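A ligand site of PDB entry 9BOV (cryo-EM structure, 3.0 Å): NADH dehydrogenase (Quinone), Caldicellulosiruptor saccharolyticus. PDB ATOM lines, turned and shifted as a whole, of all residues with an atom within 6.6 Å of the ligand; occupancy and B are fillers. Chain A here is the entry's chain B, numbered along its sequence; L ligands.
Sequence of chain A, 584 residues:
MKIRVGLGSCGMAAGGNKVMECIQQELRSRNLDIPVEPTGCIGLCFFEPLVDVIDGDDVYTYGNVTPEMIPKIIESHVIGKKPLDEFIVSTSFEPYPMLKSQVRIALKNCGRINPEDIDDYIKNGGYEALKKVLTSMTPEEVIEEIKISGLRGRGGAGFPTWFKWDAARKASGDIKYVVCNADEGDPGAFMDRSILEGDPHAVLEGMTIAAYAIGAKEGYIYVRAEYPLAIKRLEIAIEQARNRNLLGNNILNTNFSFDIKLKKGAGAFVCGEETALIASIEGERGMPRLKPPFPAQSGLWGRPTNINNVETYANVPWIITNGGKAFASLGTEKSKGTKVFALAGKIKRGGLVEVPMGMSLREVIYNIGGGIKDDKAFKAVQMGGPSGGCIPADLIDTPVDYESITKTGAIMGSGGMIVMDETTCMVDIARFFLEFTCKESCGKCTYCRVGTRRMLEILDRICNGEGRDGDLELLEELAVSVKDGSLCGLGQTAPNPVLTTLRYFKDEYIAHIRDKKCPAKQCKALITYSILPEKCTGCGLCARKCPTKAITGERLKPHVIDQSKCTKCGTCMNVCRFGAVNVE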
ATOM      1  N   VAL A 270      10.855 -20.443  -5.237  1.00  0.00           N
ATOM      2  CA  VAL A 270       9.896 -19.839  -6.140  1.00  0.00           C
ATOM      3  C   VAL A 270       8.464 -20.198  -5.786  1.00  0.00           C
ATOM      4  O   VAL A 270       7.539 -19.473  -6.157  1.00  0.00           O
ATOM      5  CB  VAL A 270      10.218 -20.225  -7.597  1.00  0.00           C
ATOM      6  CG1 VAL A 270       9.755 -21.641  -7.893  1.00  0.00           C
ATOM      7  CG2 VAL A 270       9.574 -19.248  -8.567  1.00  0.00           C
ATOM      8  N   GLU A 273       6.047 -17.564  -4.310  1.00  0.00           N
ATOM      9  CA  GLU A 273       5.314 -16.622  -5.142  1.00  0.00           C
ATOM     10  C   GLU A 273       3.842 -16.983  -5.184  1.00  0.00           C
ATOM     11  O   GLU A 273       3.470 -18.154  -5.155  1.00  0.00           O
ATOM     12  CB  GLU A 273       5.893 -16.615  -6.558  1.00  0.00           C
ATOM     13  CG  GLU A 273       5.125 -15.761  -7.534  1.00  0.00           C
ATOM     14  CD  GLU A 273       5.998 -14.790  -8.281  1.00  0.00           C
ATOM     15  OE1 GLU A 273       7.194 -15.093  -8.458  1.00  0.00           O
ATOM     16  OE2 GLU A 273       5.499 -13.725  -8.687  1.00  0.00           O
ATOM     17  N   GLY A 286       5.825 -25.620  -9.318  1.00  0.00           N
ATOM     18  CA  GLY A 286       5.730 -24.214  -8.975  1.00  0.00           C
ATOM     19  C   GLY A 286       6.285 -23.305 -10.048  1.00  0.00           C
ATOM     20  O   GLY A 286       7.340 -22.695  -9.867  1.00  0.00           O
ATOM     21  N   MET A 287       5.581 -23.195 -11.171  1.00  0.00           N
ATOM     22  CA  MET A 287       5.989 -22.321 -12.242  1.00  0.00           C
ATOM     23  C   MET A 287       5.096 -21.087 -12.241  1.00  0.00           C
ATOM     24  O   MET A 287       3.897 -21.221 -12.515  1.00  0.00           O
ATOM     25  CB  MET A 287       5.908 -23.031 -13.595  1.00  0.00           C
ATOM     26  CG  MET A 287       7.252 -23.422 -14.167  1.00  0.00           C
ATOM     27  SD  MET A 287       7.134 -24.812 -15.307  1.00  0.00           S
ATOM     28  CE  MET A 287       8.845 -24.969 -15.815  1.00  0.00           C
ATOM     29  N   PRO A 288       5.607 -19.907 -11.906  1.00  0.00           N
ATOM     30  CA  PRO A 288       4.745 -18.721 -11.854  1.00  0.00           C
ATOM     31  C   PRO A 288       4.083 -18.440 -13.199  1.00  0.00           C
ATOM     32  O   PRO A 288       4.701 -18.567 -14.257  1.00  0.00           O
ATOM     33  CB  PRO A 288       5.717 -17.597 -11.467  1.00  0.00           C
ATOM     34  CG  PRO A 288       6.821 -18.290 -10.766  1.00  0.00           C
ATOM     35  CD  PRO A 288       6.969 -19.619 -11.437  1.00  0.00           C
ATOM     36  N   ARG A 289       2.820 -18.052 -13.145  1.00  0.00           N
ATOM     37  CA  ARG A 289       2.052 -17.697 -14.324  1.00  0.00           C
ATOM     38  C   ARG A 289       2.018 -16.182 -14.464  1.00  0.00           C
ATOM     39  O   ARG A 289       2.576 -15.447 -13.645  1.00  0.00           O
ATOM     40  CB  ARG A 289       0.643 -18.288 -14.238  1.00  0.00           C
ATOM     41  CG  ARG A 289       0.617 -19.811 -14.320  1.00  0.00           C
ATOM     42  CD  ARG A 289       0.565 -20.437 -12.936  1.00  0.00           C
ATOM     43  NE  ARG A 289      -0.745 -20.300 -12.316  1.00  0.00           N
ATOM     44  CZ  ARG A 289      -1.598 -21.293 -12.145  1.00  0.00           C
ATOM     45  NH1 ARG A 289      -1.303 -22.528 -12.531  1.00  0.00           N
ATOM     46  NH2 ARG A 289      -2.773 -21.050 -11.577  1.00  0.00           N
ATOM     47  N   GLU A 440      17.572 -21.325  -7.562  1.00  0.00           N
ATOM     48  CA  GLU A 440      16.170 -21.344  -7.188  1.00  0.00           C
ATOM     49  C   GLU A 440      15.222 -20.914  -8.311  1.00  0.00           C
ATOM     50  O   GLU A 440      14.009 -20.912  -8.104  1.00  0.00           O
ATOM     51  CB  GLU A 440      15.930 -20.453  -5.961  1.00  0.00           C
ATOM     52  CG  GLU A 440      16.718 -20.874  -4.731  1.00  0.00           C
ATOM     53  CD  GLU A 440      16.487 -22.317  -4.349  1.00  0.00           C
ATOM     54  OE1 GLU A 440      15.555 -22.591  -3.561  1.00  0.00           O
ATOM     55  OE2 GLU A 440      17.247 -23.198  -4.823  1.00  0.00           O
ATOM     56  N   SER A 441      15.743 -20.557  -9.482  1.00  0.00           N
ATOM     57  CA  SER A 441      14.873 -20.212 -10.596  1.00  0.00           C
ATOM     58  C   SER A 441      14.111 -21.445 -11.076  1.00  0.00           C
ATOM     59  O   SER A 441      14.582 -22.569 -10.946  1.00  0.00           O
ATOM     60  CB  SER A 441      15.683 -19.620 -11.740  1.00  0.00           C
ATOM     61  OG  SER A 441      16.161 -20.637 -12.599  1.00  0.00           O
ATOM     62  N   CYS A 442      12.924 -21.209 -11.642  1.00  0.00           N
ATOM     63  CA  CYS A 442      12.121 -22.310 -12.160  1.00  0.00           C
ATOM     64  C   CYS A 442      12.435 -22.648 -13.607  1.00  0.00           C
ATOM     65  O   CYS A 442      12.149 -23.773 -14.040  1.00  0.00           O
ATOM     66  CB  CYS A 442      10.631 -21.986 -12.029  1.00  0.00           C
ATOM     67  SG  CYS A 442       9.922 -21.080 -13.412  1.00  0.00           S
ATOM     68  N   GLY A 443      12.998 -21.716 -14.372  1.00  0.00           N
ATOM     69  CA  GLY A 443      13.467 -22.011 -15.713  1.00  0.00           C
ATOM     70  C   GLY A 443      12.487 -21.755 -16.835  1.00  0.00           C
ATOM     71  O   GLY A 443      12.725 -22.230 -17.949  1.00  0.00           O
ATOM     72  N   LYS A 444      11.404 -21.033 -16.584  1.00  0.00           N
ATOM     73  CA  LYS A 444      10.413 -20.819 -17.638  1.00  0.00           C
ATOM     74  C   LYS A 444      10.904 -19.823 -18.673  1.00  0.00           C
ATOM     75  O   LYS A 444      10.998 -20.143 -19.863  1.00  0.00           O
ATOM     76  CB  LYS A 444       9.084 -20.370 -17.030  1.00  0.00           C
ATOM     77  CG  LYS A 444       8.116 -19.791 -18.049  1.00  0.00           C
ATOM     78  CD  LYS A 444       7.024 -18.978 -17.381  1.00  0.00           C
ATOM     79  CE  LYS A 444       5.847 -19.850 -17.007  1.00  0.00           C
ATOM     80  NZ  LYS A 444       4.608 -19.051 -16.831  1.00  0.00           N
ATOM     81  N   CYS A 445      11.228 -18.606 -18.245  1.00  0.00           N
ATOM     82  CA  CYS A 445      11.596 -17.544 -19.173  1.00  0.00           C
ATOM     83  C   CYS A 445      13.107 -17.474 -19.351  1.00  0.00           C
ATOM     84  O   CYS A 445      13.877 -17.770 -18.438  1.00  0.00           O
ATOM     85  CB  CYS A 445      11.060 -16.186 -18.707  1.00  0.00           C
ATOM     86  SG  CYS A 445      11.501 -15.742 -17.027  1.00  0.00           S
ATOM     87  N   THR A 446      13.529 -17.050 -20.545  1.00  0.00           N
ATOM     88  CA  THR A 446      14.938 -17.067 -20.900  1.00  0.00           C
ATOM     89  C   THR A 446      15.757 -16.123 -20.015  1.00  0.00           C
ATOM     90  O   THR A 446      16.870 -16.459 -19.604  1.00  0.00           O
ATOM     91  CB  THR A 446      15.122 -16.713 -22.370  1.00  0.00           C
ATOM     92  OG1 THR A 446      16.511 -16.466 -22.633  1.00  0.00           O
ATOM     93  CG2 THR A 446      14.315 -15.483 -22.736  1.00  0.00           C
ATOM     94  N   TYR A 447      15.214 -14.943 -19.721  1.00  0.00           N
ATOM     95  CA  TYR A 447      16.002 -13.935 -19.008  1.00  0.00           C
ATOM     96  C   TYR A 447      16.439 -14.418 -17.633  1.00  0.00           C
ATOM     97  O   TYR A 447      17.578 -14.195 -17.224  1.00  0.00           O
ATOM     98  CB  TYR A 447      15.195 -12.645 -18.894  1.00  0.00           C
ATOM     99  CG  TYR A 447      15.096 -11.858 -20.164  1.00  0.00           C
ATOM    100  CD1 TYR A 447      16.234 -11.386 -20.806  1.00  0.00           C
ATOM    101  CD2 TYR A 447      13.866 -11.574 -20.732  1.00  0.00           C
ATOM    102  CE1 TYR A 447      16.145 -10.664 -21.976  1.00  0.00           C
ATOM    103  CE2 TYR A 447      13.764 -10.849 -21.906  1.00  0.00           C
ATOM    104  CZ  TYR A 447      14.911 -10.398 -22.520  1.00  0.00           C
ATOM    105  OH  TYR A 447      14.814  -9.666 -23.683  1.00  0.00           O
ATOM    106  N   CYS A 448      15.547 -15.091 -16.906  1.00  0.00           N
ATOM    107  CA  CYS A 448      15.920 -15.555 -15.576  1.00  0.00           C
ATOM    108  C   CYS A 448      16.635 -16.908 -15.623  1.00  0.00           C
ATOM    109  O   CYS A 448      17.531 -17.145 -14.809  1.00  0.00           O
ATOM    110  CB  CYS A 448      14.687 -15.659 -14.683  1.00  0.00           C
ATOM    111  SG  CYS A 448      14.978 -16.501 -13.105  1.00  0.00           S
ATOM    112  N   ARG A 449      16.250 -17.786 -16.540  1.00  0.00           N
ATOM    113  CA  ARG A 449      16.798 -19.142 -16.533  1.00  0.00           C
ATOM    114  C   ARG A 449      18.269 -19.150 -16.923  1.00  0.00           C
ATOM    115  O   ARG A 449      19.100 -19.766 -16.250  1.00  0.00           O
ATOM    116  CB  ARG A 449      15.997 -20.044 -17.462  1.00  0.00           C
ATOM    117  CG  ARG A 449      16.516 -21.460 -17.538  1.00  0.00           C
ATOM    118  CD  ARG A 449      15.897 -22.221 -18.692  1.00  0.00           C
ATOM    119  NE  ARG A 449      16.275 -21.663 -19.979  1.00  0.00           N
ATOM    120  CZ  ARG A 449      15.410 -21.270 -20.909  1.00  0.00           C
ATOM    121  NH1 ARG A 449      14.106 -21.365 -20.723  1.00  0.00           N
ATOM    122  NH2 ARG A 449      15.876 -20.780 -22.058  1.00  0.00           N
ATOM    123  N   SER A 486      12.550 -10.325 -17.133  1.00  0.00           N
ATOM    124  CA  SER A 486      12.095 -11.556 -16.490  1.00  0.00           C
ATOM    125  C   SER A 486      10.590 -11.494 -16.228  1.00  0.00           C
ATOM    126  O   SER A 486       9.995 -10.422 -16.111  1.00  0.00           O
ATOM    127  CB  SER A 486      12.853 -11.801 -15.196  1.00  0.00           C
ATOM    128  OG  SER A 486      14.245 -11.815 -15.418  1.00  0.00           O
ATOM    129  N   LEU A 487       9.978 -12.674 -16.115  1.00  0.00           N
ATOM    130  CA  LEU A 487       8.528 -12.750 -15.980  1.00  0.00           C
ATOM    131  C   LEU A 487       8.097 -12.507 -14.542  1.00  0.00           C
ATOM    132  O   LEU A 487       7.311 -11.596 -14.274  1.00  0.00           O
ATOM    133  CB  LEU A 487       8.037 -14.120 -16.464  1.00  0.00           C
ATOM    134  CG  LEU A 487       6.545 -14.308 -16.727  1.00  0.00           C
ATOM    135  CD1 LEU A 487       6.332 -15.398 -17.762  1.00  0.00           C
ATOM    136  CD2 LEU A 487       5.798 -14.668 -15.447  1.00  0.00           C
ATOM    137  N   CYS A 488       8.595 -13.302 -13.611  1.00  0.00           N
ATOM    138  CA  CYS A 488       8.142 -13.250 -12.229  1.00  0.00           C
ATOM    139  C   CYS A 488       9.086 -12.409 -11.392  1.00  0.00           C
ATOM    140  O   CYS A 488      10.075 -11.847 -11.885  1.00  0.00           O
ATOM    141  CB  CYS A 488       8.011 -14.662 -11.661  1.00  0.00           C
ATOM    142  SG  CYS A 488       9.472 -15.231 -10.784  1.00  0.00           S
ATOM    143  N   GLY A 489       8.769 -12.299 -10.095  1.00  0.00           N
ATOM    144  CA  GLY A 489       9.572 -11.482  -9.202  1.00  0.00           C
ATOM    145  C   GLY A 489      10.886 -12.091  -8.792  1.00  0.00           C
ATOM    146  O   GLY A 489      11.744 -11.383  -8.244  1.00  0.00           O
ATOM    147  N   LEU A 490      11.070 -13.390  -9.019  1.00  0.00           N
ATOM    148  CA  LEU A 490      12.352 -14.016  -8.701  1.00  0.00           C
ATOM    149  C   LEU A 490      13.424 -13.662  -9.715  1.00  0.00           C
ATOM    150  O   LEU A 490      14.616 -13.788  -9.414  1.00  0.00           O
ATOM    151  CB  LEU A 490      12.192 -15.536  -8.602  1.00  0.00           C
ATOM    152  CG  LEU A 490      13.408 -16.363  -8.202  1.00  0.00           C
ATOM    153  CD1 LEU A 490      14.015 -15.828  -6.924  1.00  0.00           C
ATOM    154  CD2 LEU A 490      13.023 -17.818  -8.039  1.00  0.00           C
ATOM    155  N   GLY A 491      13.031 -13.230 -10.906  1.00  0.00           N
ATOM    156  CA  GLY A 491      13.983 -12.807 -11.908  1.00  0.00           C
ATOM    157  C   GLY A 491      14.139 -11.301 -11.941  1.00  0.00           C
ATOM    158  O   GLY A 491      15.232 -10.789 -12.178  1.00  0.00           O
ATOM    159  N   GLN A 492      13.039 -10.590 -11.694  1.00  0.00           N
ATOM    160  CA  GLN A 492      13.104  -9.132 -11.652  1.00  0.00           C
ATOM    161  C   GLN A 492      13.885  -8.642 -10.437  1.00  0.00           C
ATOM    162  O   GLN A 492      14.412  -7.526 -10.458  1.00  0.00           O
ATOM    163  CB  GLN A 492      11.694  -8.541 -11.641  1.00  0.00           C
ATOM    164  CG  GLN A 492      10.905  -8.821 -12.899  1.00  0.00           C
ATOM    165  CD  GLN A 492       9.460  -8.378 -12.776  1.00  0.00           C
ATOM    166  OE1 GLN A 492       9.019  -7.966 -11.715  1.00  0.00           O
ATOM    167  NE2 GLN A 492       8.715  -8.475 -13.872  1.00  0.00           N
HETATM  168 FE1  LIG L   1      10.694 -18.961 -13.492  1.00  0.00          FE
HETATM  169 FE2  LIG L   1      11.056 -16.755 -15.076  1.00  0.00          FE
HETATM  170 FE3  LIG L   1      12.897 -17.372 -13.160  1.00  0.00          FE
HETATM  171 FE4  LIG L   1      10.430 -16.451 -12.432  1.00  0.00          FE
HETATM  172  S1  LIG L   1      12.022 -15.323 -13.597  1.00  0.00           S
HETATM  173  S2  LIG L   1      11.557 -18.214 -11.520  1.00  0.00           S
HETATM  174  S3  LIG L   1       9.131 -17.398 -14.047  1.00  0.00           S
HETATM  175  S4  LIG L   1      12.372 -18.613 -14.993  1.00  0.00           S
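Residues that only touch the ligand: Val 270, Leu 490, Ser 441 and Ser 486.
Hydrophobic or aromatic side chains within 4 Å of the ligand: Val 270 and Leu 490.
11 residues have an atom within 4 Å of the ligand: Val 270, Ser 441, Cys 442, Gly 443, Lys 444, Cys 445, Cys 448, Ser 486, Cys 488, Leu 490 and Gly 491.
N of Cys 445 lies close to S4 of the ligand (3.4 Å).
The side-chain sulfur (SG) of Cys 445 binds an iron atom (FE2) of the ligand (2.2 Å).
N of Cys 442 lies close to S2 of the ligand (3.3 Å).
An iron atom (FE1) of the ligand is bound by the side-chain sulfur (SG) of Cys 442, at 2.3 Å.
SG of Cys 448 binds FE3 of the ligand.
FE4 of the ligand is bound by SG of Cys 488.
A sulfur (S4) of the ligand lies close to the backbone NH (N) of Lys 444 (3.1 Å).
N of Gly 443 lies close to S4 of the ligand (3.2 Å).
The backbone NH (N) of Gly 491 lies close to a sulfur (S1) of the ligand.
SG of Cys 445 sits close to N of Leu 487 (3.5 Å).
The backbone NH of Lys 444 lies close to the side-chain sulfur of Cys 442.
The side-chain sulfur (SG) of Cys 488 lies close to the backbone NH (N) of Leu 490 (3.0 Å).
The side-chain sulfur (SG) of Cys 488 lies close to the side-chain carboxylate (OE1) of Glu 273 (3.3 Å).
NZ of Lys 444 sits at hydrogen-bond distance from O of Pro 288, 2.6 Å away.
The backbone carbonyl oxygen (O) of Lys 444 is in hydrogen-bond range of the guanidinium group (NH1) of Arg 449, at 3.4 Å.
O of Gly 443 sits at hydrogen-bond distance from NH1 of Arg 449, 3.2 Å away.
The backbone carbonyl oxygen (O) of Ser 486 sits at hydrogen-bond distance from the side-chain amide nitrogen (NE2) of Gln 492, at 3.2 Å.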
